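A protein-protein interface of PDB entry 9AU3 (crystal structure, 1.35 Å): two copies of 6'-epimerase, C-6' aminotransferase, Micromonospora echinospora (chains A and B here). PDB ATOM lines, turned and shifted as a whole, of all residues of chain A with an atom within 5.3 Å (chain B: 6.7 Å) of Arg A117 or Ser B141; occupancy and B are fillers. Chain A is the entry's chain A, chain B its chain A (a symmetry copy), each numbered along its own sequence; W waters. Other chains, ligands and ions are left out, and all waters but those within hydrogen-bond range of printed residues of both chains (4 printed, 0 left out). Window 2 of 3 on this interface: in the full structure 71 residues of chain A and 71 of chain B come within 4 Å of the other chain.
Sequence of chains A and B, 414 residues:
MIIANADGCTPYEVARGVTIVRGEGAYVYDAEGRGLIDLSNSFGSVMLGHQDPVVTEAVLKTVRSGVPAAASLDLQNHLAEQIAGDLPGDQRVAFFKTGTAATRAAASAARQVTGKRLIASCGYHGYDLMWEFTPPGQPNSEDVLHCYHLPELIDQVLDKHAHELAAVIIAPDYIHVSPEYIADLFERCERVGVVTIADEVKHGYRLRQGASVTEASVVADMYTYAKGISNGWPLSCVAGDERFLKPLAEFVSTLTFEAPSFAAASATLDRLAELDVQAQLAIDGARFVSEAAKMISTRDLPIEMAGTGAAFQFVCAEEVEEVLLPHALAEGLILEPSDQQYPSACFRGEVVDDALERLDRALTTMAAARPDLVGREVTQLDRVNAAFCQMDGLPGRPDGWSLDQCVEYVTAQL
Of the printed residues of chain B, Arg A117 touches Arg B117, Ser B141 and Glu B142. Printed residues of chain A within 4 Å of Ser B141: Arg A117 (3.6 Å). Printed residues of chain B within 4 Å of Arg A111: Glu B142 (3.9 Å). Printed residues of chain B within 4 Å of Ser A141: Arg B117 (3.6 Å). Printed residues of chain B within 4 Å of Glu A142: Arg B117 (3.0 Å) and Glu B142 (3.4 Å). Of the printed residues of chain A, Glu B142 touches Arg A111 (3.9 Å), Arg A117 (3.0 Å) and Glu A142 (3.4 Å). The nearest residue of chain B that does not touch Arg A117 is Asp B143 (5.9 Å). The nearest printed residue of chain A that does not touch Ser B141 is Glu A142 (6.7 Å). The nearest printed residue of chain B that does not touch Arg A111 is Leu B129 (5.6 Å).
The guanidinium group (NE) of Arg A111 sits at hydrogen-bond distance from the backbone carbonyl oxygen (O) of Arg A117 (2.8 Å). The guanidinium group of Arg B117 is in salt-bridge range of the side-chain carboxylate of Asp B143 (2.8 Å). The backbone carbonyl oxygen (O) of Glu A142 lies within hydrogen-bond range of the guanidinium group (NH2) of Arg A111, 2.8 Å away. The side-chain carboxylate (OD2) of Asp A143 lies within salt-bridge range of the guanidinium group (NE) of Arg A117 (2.8 Å). The guanidinium group (NH2) of Arg A117 is in salt-bridge range of the side-chain carboxylate (OE1) of Glu A142. OD1 of Asn B140 lies within hydrogen-bond range of N of Glu B142, 3.0 Å away.
Arg B117 touches its own counterpart, Arg A117. Arg A117 touches Ser B141, and with the chains exchanged Ser A141 touches Arg B117. Arg A117 touches Glu B142, and with the chains exchanged Glu A142 touches Arg B117. Glu A142 touches its own counterpart, Glu B142.
NH1 of Arg A111 is in salt-bridge range of OE2 of Glu B142. The side-chain carboxylate of Glu A142 lies close to the side-chain carboxylate of Glu B142 (3.4 Å). The side-chain carboxylate (OE1) of Glu A142 lies within salt-bridge range of the guanidinium group (NH2) of Arg B117 (3.0 Å). The side-chain carboxylate (OE1) of Glu B142 is in salt-bridge range of the guanidinium group (NH2) of Arg A117 (3.0 Å). NH2 of Arg A117 sits close to NH2 of Arg B117, 3.4 Å away.
Among the printed residues, merely in contact across the chains: Arg A117 with Ser B141 (3.6 Å) and Ser A141 with Arg B117 (3.6 Å).
Water W2 lies within hydrogen-bond range of the side-chain carboxylate of Glu A142, the side-chain carboxylate of Glu B142 and the guanidinium group of Arg B117. Water W3 lies within hydrogen-bond range of OE2 of Glu B142 (2.7 Å), OE1 of Glu A142 (2.8 Å), NH1 of Arg A111 (2.9 Å) and NH2 of Arg A117 (3.3 Å). Water W1 lies within hydrogen-bond range of the side-chain carboxylate (OD2) of Asp A143, the backbone carbonyl oxygen (O) of Ser A141, the guanidinium group (NH2) of Arg A117 and the guanidinium group (NH2) of Arg B117. Water W4 lies within hydrogen-bond range of the side-chain carboxylate of Asp B143 (2.8 Å), the backbone carbonyl oxygen of Ser B141 (2.9 Å), the guanidinium group of Arg B117 (3.0 Å) and the guanidinium group of Arg A117 (3.4 Å).
Of the 11 printed residues of chain B, 3 touch a printed residue of chain A. Printed residues of chain B that touch a printed residue of chain A: Arg B117, Ser B141 and Glu B142. Among the printed residues, 7 pairs touch across the chains. Among the printed residues, Asp or Glu carboxylates within 4 Å of a Lys or Arg side-chain nitrogen of the other chain: Arg A111 with Glu B142, Arg A117 with Glu B142 and Glu A142 with Arg B117.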
ATOM      1  N   ARG A 111     -30.775  -2.044  14.359  1.00  0.00           N
ATOM      2  CA  ARG A 111     -31.654  -2.325  15.490  1.00  0.00           C
ATOM      3  C   ARG A 111     -32.735  -1.256  15.630  1.00  0.00           C
ATOM      4  O   ARG A 111     -33.906  -1.576  15.861  1.00  0.00           O
ATOM      5  CB  ARG A 111     -30.812  -2.425  16.758  1.00  0.00           C
ATOM      6  CG  ARG A 111     -29.982  -3.703  16.822  1.00  0.00           C
ATOM      7  CD  ARG A 111     -29.077  -3.701  18.028  1.00  0.00           C
ATOM      8  NE  ARG A 111     -28.539  -5.032  18.273  1.00  0.00           N
ATOM      9  CZ  ARG A 111     -27.590  -5.313  19.155  1.00  0.00           C
ATOM     10  NH1 ARG A 111     -26.923  -4.351  19.784  1.00  0.00           N
ATOM     11  NH2 ARG A 111     -27.307  -6.589  19.415  1.00  0.00           N
ATOM     12  N   GLY A 115     -36.398  -2.622  14.927  1.00  0.00           N
ATOM     13  CA  GLY A 115     -36.916  -2.972  16.230  1.00  0.00           C
ATOM     14  C   GLY A 115     -36.509  -4.340  16.725  1.00  0.00           C
ATOM     15  O   GLY A 115     -37.081  -4.821  17.711  1.00  0.00           O
ATOM     16  N   LYS A 116     -35.551  -4.989  16.070  1.00  0.00           N
ATOM     17  CA  LYS A 116     -35.053  -6.292  16.478  1.00  0.00           C
ATOM     18  C   LYS A 116     -33.672  -6.135  17.098  1.00  0.00           C
ATOM     19  O   LYS A 116     -33.019  -5.100  16.959  1.00  0.00           O
ATOM     20  CB  LYS A 116     -35.008  -7.259  15.289  1.00  0.00           C
ATOM     21  CG  LYS A 116     -36.381  -7.579  14.725  1.00  0.00           C
ATOM     22  CD  LYS A 116     -36.303  -7.889  13.246  1.00  0.00           C
ATOM     23  CE  LYS A 116     -37.687  -8.184  12.676  1.00  0.00           C
ATOM     24  NZ  LYS A 116     -37.634  -8.562  11.237  1.00  0.00           N
ATOM     25  N   ARG A 117     -33.221  -7.180  17.783  1.00  0.00           N
ATOM     26  CA  ARG A 117     -31.981  -7.094  18.545  1.00  0.00           C
ATOM     27  C   ARG A 117     -30.878  -8.012  18.040  1.00  0.00           C
ATOM     28  O   ARG A 117     -29.722  -7.587  17.948  1.00  0.00           O
ATOM     29  CB  ARG A 117     -32.264  -7.396  20.020  1.00  0.00           C
ATOM     30  CG  ARG A 117     -31.018  -7.604  20.847  1.00  0.00           C
ATOM     31  CD  ARG A 117     -30.986  -6.650  21.991  1.00  0.00           C
ATOM     32  NE  ARG A 117     -29.718  -6.687  22.706  1.00  0.00           N
ATOM     33  CZ  ARG A 117     -29.011  -5.608  23.008  1.00  0.00           C
ATOM     34  NH1 ARG A 117     -29.369  -4.407  22.583  1.00  0.00           N
ATOM     35  NH2 ARG A 117     -27.916  -5.736  23.753  1.00  0.00           N
ATOM     36  N   LEU A 118     -31.202  -9.255  17.698  1.00  0.00           N
ATOM     37  CA  LEU A 118     -30.183 -10.235  17.349  1.00  0.00           C
ATOM     38  C   LEU A 118     -29.456  -9.821  16.072  1.00  0.00           C
ATOM     39  O   LEU A 118     -30.069  -9.332  15.119  1.00  0.00           O
ATOM     40  CB  LEU A 118     -30.865 -11.587  17.152  1.00  0.00           C
ATOM     41  CG  LEU A 118     -30.058 -12.883  17.170  1.00  0.00           C
ATOM     42  CD1 LEU A 118     -29.456 -13.143  18.555  1.00  0.00           C
ATOM     43  CD2 LEU A 118     -30.981 -14.016  16.768  1.00  0.00           C
ATOM     44  N   ILE A 119     -28.139 -10.019  16.055  1.00  0.00           N
ATOM     45  CA  ILE A 119     -27.302  -9.736  14.890  1.00  0.00           C
ATOM     46  C   ILE A 119     -26.502 -10.987  14.579  1.00  0.00           C
ATOM     47  O   ILE A 119     -26.000 -11.647  15.497  1.00  0.00           O
ATOM     48  CB  ILE A 119     -26.334  -8.562  15.176  1.00  0.00           C
ATOM     49  CG1 ILE A 119     -27.101  -7.274  15.493  1.00  0.00           C
ATOM     50  CG2 ILE A 119     -25.275  -8.406  14.061  1.00  0.00           C
ATOM     51  CD1 ILE A 119     -27.284  -6.358  14.350  1.00  0.00           C
ATOM     52  N   SER A 141     -22.712 -11.789  24.704  1.00  0.00           N
ATOM     53  CA  SER A 141     -23.370 -11.003  25.746  1.00  0.00           C
ATOM     54  C   SER A 141     -24.185  -9.849  25.189  1.00  0.00           C
ATOM     55  O   SER A 141     -25.018  -9.290  25.916  1.00  0.00           O
ATOM     56  CB  SER A 141     -22.340 -10.473  26.749  1.00  0.00           C
ATOM     57  OG  SER A 141     -21.581  -9.406  26.212  1.00  0.00           O
ATOM     58  N   GLU A 142     -23.966  -9.481  23.927  1.00  0.00           N
ATOM     59  CA  GLU A 142     -24.696  -8.404  23.282  1.00  0.00           C
ATOM     60  C   GLU A 142     -25.598  -8.922  22.168  1.00  0.00           C
ATOM     61  O   GLU A 142     -25.971  -8.156  21.273  1.00  0.00           O
ATOM     62  CB  GLU A 142     -23.725  -7.351  22.741  1.00  0.00           C
ATOM     63  CG  GLU A 142     -22.902  -6.649  23.823  1.00  0.00           C
ATOM     64  CD  GLU A 142     -23.718  -5.688  24.668  1.00  0.00           C
ATOM     65  OE1 GLU A 142     -24.962  -5.646  24.552  1.00  0.00           O
ATOM     66  OE2 GLU A 142     -23.107  -4.963  25.471  1.00  0.00           O
ATOM     67  N   ASP A 143     -25.919 -10.222  22.185  1.00  0.00           N
ATOM     68  CA  ASP A 143     -26.889 -10.819  21.262  1.00  0.00           C
ATOM     69  C   ASP A 143     -26.383 -10.841  19.818  1.00  0.00           C
ATOM     70  O   ASP A 143     -27.131 -10.575  18.870  1.00  0.00           O
ATOM     71  CB  ASP A 143     -28.263 -10.161  21.391  1.00  0.00           C
ATOM     72  CG  ASP A 143     -28.837 -10.336  22.776  1.00  0.00           C
ATOM     73  OD1 ASP A 143     -28.847 -11.484  23.260  1.00  0.00           O
ATOM     74  OD2 ASP A 143     -29.235  -9.331  23.401  1.00  0.00           O
ATOM     75  N   GLU A 164     -35.995 -12.771  13.266  1.00  0.00           N
ATOM     76  CA  GLU A 164     -35.579 -12.124  14.499  1.00  0.00           C
ATOM     77  C   GLU A 164     -34.348 -11.249  14.324  1.00  0.00           C
ATOM     78  O   GLU A 164     -33.974 -10.538  15.264  1.00  0.00           O
ATOM     79  CB  GLU A 164     -35.235 -13.205  15.532  1.00  0.00           C
ATOM     80  CG  GLU A 164     -36.426 -13.871  16.168  1.00  0.00           C
ATOM     81  CD  GLU A 164     -36.065 -14.553  17.462  1.00  0.00           C
ATOM     82  OE1 GLU A 164     -35.360 -15.586  17.407  1.00  0.00           O
ATOM     83  OE2 GLU A 164     -36.479 -14.059  18.530  1.00  0.00           O
ATOM     84  N   ALA A 166     -31.895  -8.323  13.353  1.00  0.00           N
ATOM     85  CA  ALA A 166     -31.821  -6.927  12.939  1.00  0.00           C
ATOM     86  C   ALA A 166     -30.948  -6.769  11.703  1.00  0.00           C
ATOM     87  O   ALA A 166     -31.239  -5.935  10.838  1.00  0.00           O
ATOM     88  CB  ALA A 166     -31.268  -6.069  14.077  1.00  0.00           C
ATOM     89  N   ARG B 117     -25.173  -6.959  34.650  1.00  0.00           N
ATOM     90  CA  ARG B 117     -25.466  -6.223  33.427  1.00  0.00           C
ATOM     91  C   ARG B 117     -26.014  -4.823  33.659  1.00  0.00           C
ATOM     92  O   ARG B 117     -25.593  -3.881  32.982  1.00  0.00           O
ATOM     93  CB  ARG B 117     -26.454  -7.025  32.573  1.00  0.00           C
ATOM     94  CG  ARG B 117     -27.036  -6.239  31.421  1.00  0.00           C
ATOM     95  CD  ARG B 117     -26.766  -6.932  30.129  1.00  0.00           C
ATOM     96  NE  ARG B 117     -27.144  -6.122  28.979  1.00  0.00           N
ATOM     97  CZ  ARG B 117     -26.348  -5.898  27.943  1.00  0.00           C
ATOM     98  NH1 ARG B 117     -25.094  -6.322  27.931  1.00  0.00           N
ATOM     99  NH2 ARG B 117     -26.821  -5.230  26.894  1.00  0.00           N
ATOM    100  N   LEU B 129     -26.170   4.185  22.094  1.00  0.00           N
ATOM    101  CA  LEU B 129     -27.520   3.876  22.560  1.00  0.00           C
ATOM    102  C   LEU B 129     -27.555   3.455  24.025  1.00  0.00           C
ATOM    103  O   LEU B 129     -28.584   3.607  24.683  1.00  0.00           O
ATOM    104  CB  LEU B 129     -28.125   2.767  21.692  1.00  0.00           C
ATOM    105  CG  LEU B 129     -28.578   3.235  20.317  1.00  0.00           C
ATOM    106  CD1 LEU B 129     -29.297   2.118  19.585  1.00  0.00           C
ATOM    107  CD2 LEU B 129     -29.476   4.472  20.459  1.00  0.00           C
ATOM    108  N   MET B 130     -26.455   2.924  24.558  1.00  0.00           N
ATOM    109  CA  MET B 130     -26.431   2.592  25.976  1.00  0.00           C
ATOM    110  C   MET B 130     -26.619   3.815  26.856  1.00  0.00           C
ATOM    111  O   MET B 130     -27.071   3.680  28.001  1.00  0.00           O
ATOM    112  CB  MET B 130     -25.169   1.780  26.262  1.00  0.00           C
ATOM    113  CG  MET B 130     -23.986   2.607  26.718  1.00  0.00           C
ATOM    114  SD  MET B 130     -22.613   1.585  27.200  1.00  0.00           S
ATOM    115  CE  MET B 130     -23.257   0.763  28.669  1.00  0.00           C
ATOM    116  N   GLU B 132     -28.602   6.468  25.981  1.00  0.00           N
ATOM    117  CA  GLU B 132     -29.841   7.152  25.640  1.00  0.00           C
ATOM    118  C   GLU B 132     -30.732   7.265  26.877  1.00  0.00           C
ATOM    119  O   GLU B 132     -30.993   6.279  27.567  1.00  0.00           O
ATOM    120  CB  GLU B 132     -30.549   6.391  24.520  1.00  0.00           C
ATOM    121  CG  GLU B 132     -32.031   6.758  24.320  1.00  0.00           C
ATOM    122  CD  GLU B 132     -32.713   5.920  23.257  1.00  0.00           C
ATOM    123  OE1 GLU B 132     -32.486   4.696  23.209  1.00  0.00           O
ATOM    124  OE2 GLU B 132     -33.552   6.478  22.517  1.00  0.00           O
ATOM    125  N   THR B 134     -33.823   7.466  29.295  1.00  0.00           N
ATOM    126  CA  THR B 134     -35.194   7.002  29.441  1.00  0.00           C
ATOM    127  C   THR B 134     -35.708   7.498  30.785  1.00  0.00           C
ATOM    128  O   THR B 134     -34.915   7.918  31.638  1.00  0.00           O
ATOM    129  CB  THR B 134     -35.250   5.466  29.356  1.00  0.00           C
ATOM    130  OG1 THR B 134     -34.199   4.887  30.139  1.00  0.00           O
ATOM    131  CG2 THR B 134     -35.108   4.999  27.899  1.00  0.00           C
ATOM    132  N   PRO B 139     -35.417   0.917  32.348  1.00  0.00           N
ATOM    133  CA  PRO B 139     -34.116   0.629  31.738  1.00  0.00           C
ATOM    134  C   PRO B 139     -34.196   0.832  30.234  1.00  0.00           C
ATOM    135  O   PRO B 139     -35.206   0.514  29.601  1.00  0.00           O
ATOM    136  CB  PRO B 139     -33.873  -0.846  32.087  1.00  0.00           C
ATOM    137  CG  PRO B 139     -34.805  -1.145  33.230  1.00  0.00           C
ATOM    138  CD  PRO B 139     -36.013  -0.268  32.990  1.00  0.00           C
ATOM    139  N   ASN B 140     -33.131   1.393  29.666  1.00  0.00           N
ATOM    140  CA  ASN B 140     -33.093   1.612  28.226  1.00  0.00           C
ATOM    141  C   ASN B 140     -32.750   0.303  27.512  1.00  0.00           C
ATOM    142  O   ASN B 140     -32.654  -0.761  28.129  1.00  0.00           O
ATOM    143  CB  ASN B 140     -32.220   2.816  27.862  1.00  0.00           C
ATOM    144  CG  ASN B 140     -30.735   2.550  28.014  1.00  0.00           C
ATOM    145  OD1 ASN B 140     -30.301   1.414  28.198  1.00  0.00           O
ATOM    146  ND2 ASN B 140     -29.942   3.609  27.917  1.00  0.00           N
ATOM    147  N   SER B 141     -32.538   0.377  26.194  1.00  0.00           N
ATOM    148  CA  SER B 141     -32.368  -0.832  25.390  1.00  0.00           C
ATOM    149  C   SER B 141     -31.093  -1.587  25.723  1.00  0.00           C
ATOM    150  O   SER B 141     -30.966  -2.758  25.340  1.00  0.00           O
ATOM    151  CB  SER B 141     -32.394  -0.490  23.897  1.00  0.00           C
ATOM    152  OG  SER B 141     -31.198   0.139  23.478  1.00  0.00           O
ATOM    153  N   GLU B 142     -30.152  -0.948  26.418  1.00  0.00           N
ATOM    154  CA  GLU B 142     -28.900  -1.572  26.808  1.00  0.00           C
ATOM    155  C   GLU B 142     -28.809  -1.758  28.318  1.00  0.00           C
ATOM    156  O   GLU B 142     -27.704  -1.889  28.855  1.00  0.00           O
ATOM    157  CB  GLU B 142     -27.713  -0.753  26.294  1.00  0.00           C
ATOM    158  CG  GLU B 142     -27.629  -0.668  24.769  1.00  0.00           C
ATOM    159  CD  GLU B 142     -27.210  -1.973  24.118  1.00  0.00           C
ATOM    160  OE1 GLU B 142     -27.122  -3.018  24.799  1.00  0.00           O
ATOM    161  OE2 GLU B 142     -26.969  -1.960  22.899  1.00  0.00           O
ATOM    162  N   ASP B 143     -29.951  -1.727  29.016  1.00  0.00           N
ATOM    163  CA  ASP B 143     -30.023  -2.034  30.448  1.00  0.00           C
ATOM    164  C   ASP B 143     -29.332  -0.973  31.307  1.00  0.00           C
ATOM    165  O   ASP B 143     -28.638  -1.286  32.282  1.00  0.00           O
ATOM    166  CB  ASP B 143     -29.519  -3.446  30.744  1.00  0.00           C
ATOM    167  CG  ASP B 143     -30.353  -4.494  30.046  1.00  0.00           C
ATOM    168  OD1 ASP B 143     -31.591  -4.428  30.172  1.00  0.00           O
ATOM    169  OD2 ASP B 143     -29.786  -5.351  29.339  1.00  0.00           O
ATOM    170  N   VAL B 144     -29.553   0.290  30.962  1.00  0.00           N
ATOM    171  CA  VAL B 144     -29.056   1.420  31.737  1.00  0.00           C
ATOM    172  C   VAL B 144     -30.249   2.176  32.301  1.00  0.00           C
ATOM    173  O   VAL B 144     -31.192   2.490  31.563  1.00  0.00           O
ATOM    174  CB  VAL B 144     -28.158   2.335  30.887  1.00  0.00           C
ATOM    175  CG1 VAL B 144     -27.728   3.570  31.688  1.00  0.00           C
ATOM    176  CG2 VAL B 144     -26.952   1.556  30.384  1.00  0.00           C
HETATM  177  O   HOH W   1     -27.631  -8.237  25.472  1.00  0.00           O
HETATM  178  O   HOH W   2     -24.649  -2.835  26.153  1.00  0.00           O
HETATM  179  O   HOH W   3     -25.456  -4.114  22.231  1.00  0.00           O
HETATM  180  O   HOH W   4     -29.842  -5.103  26.511  1.00  0.00           O
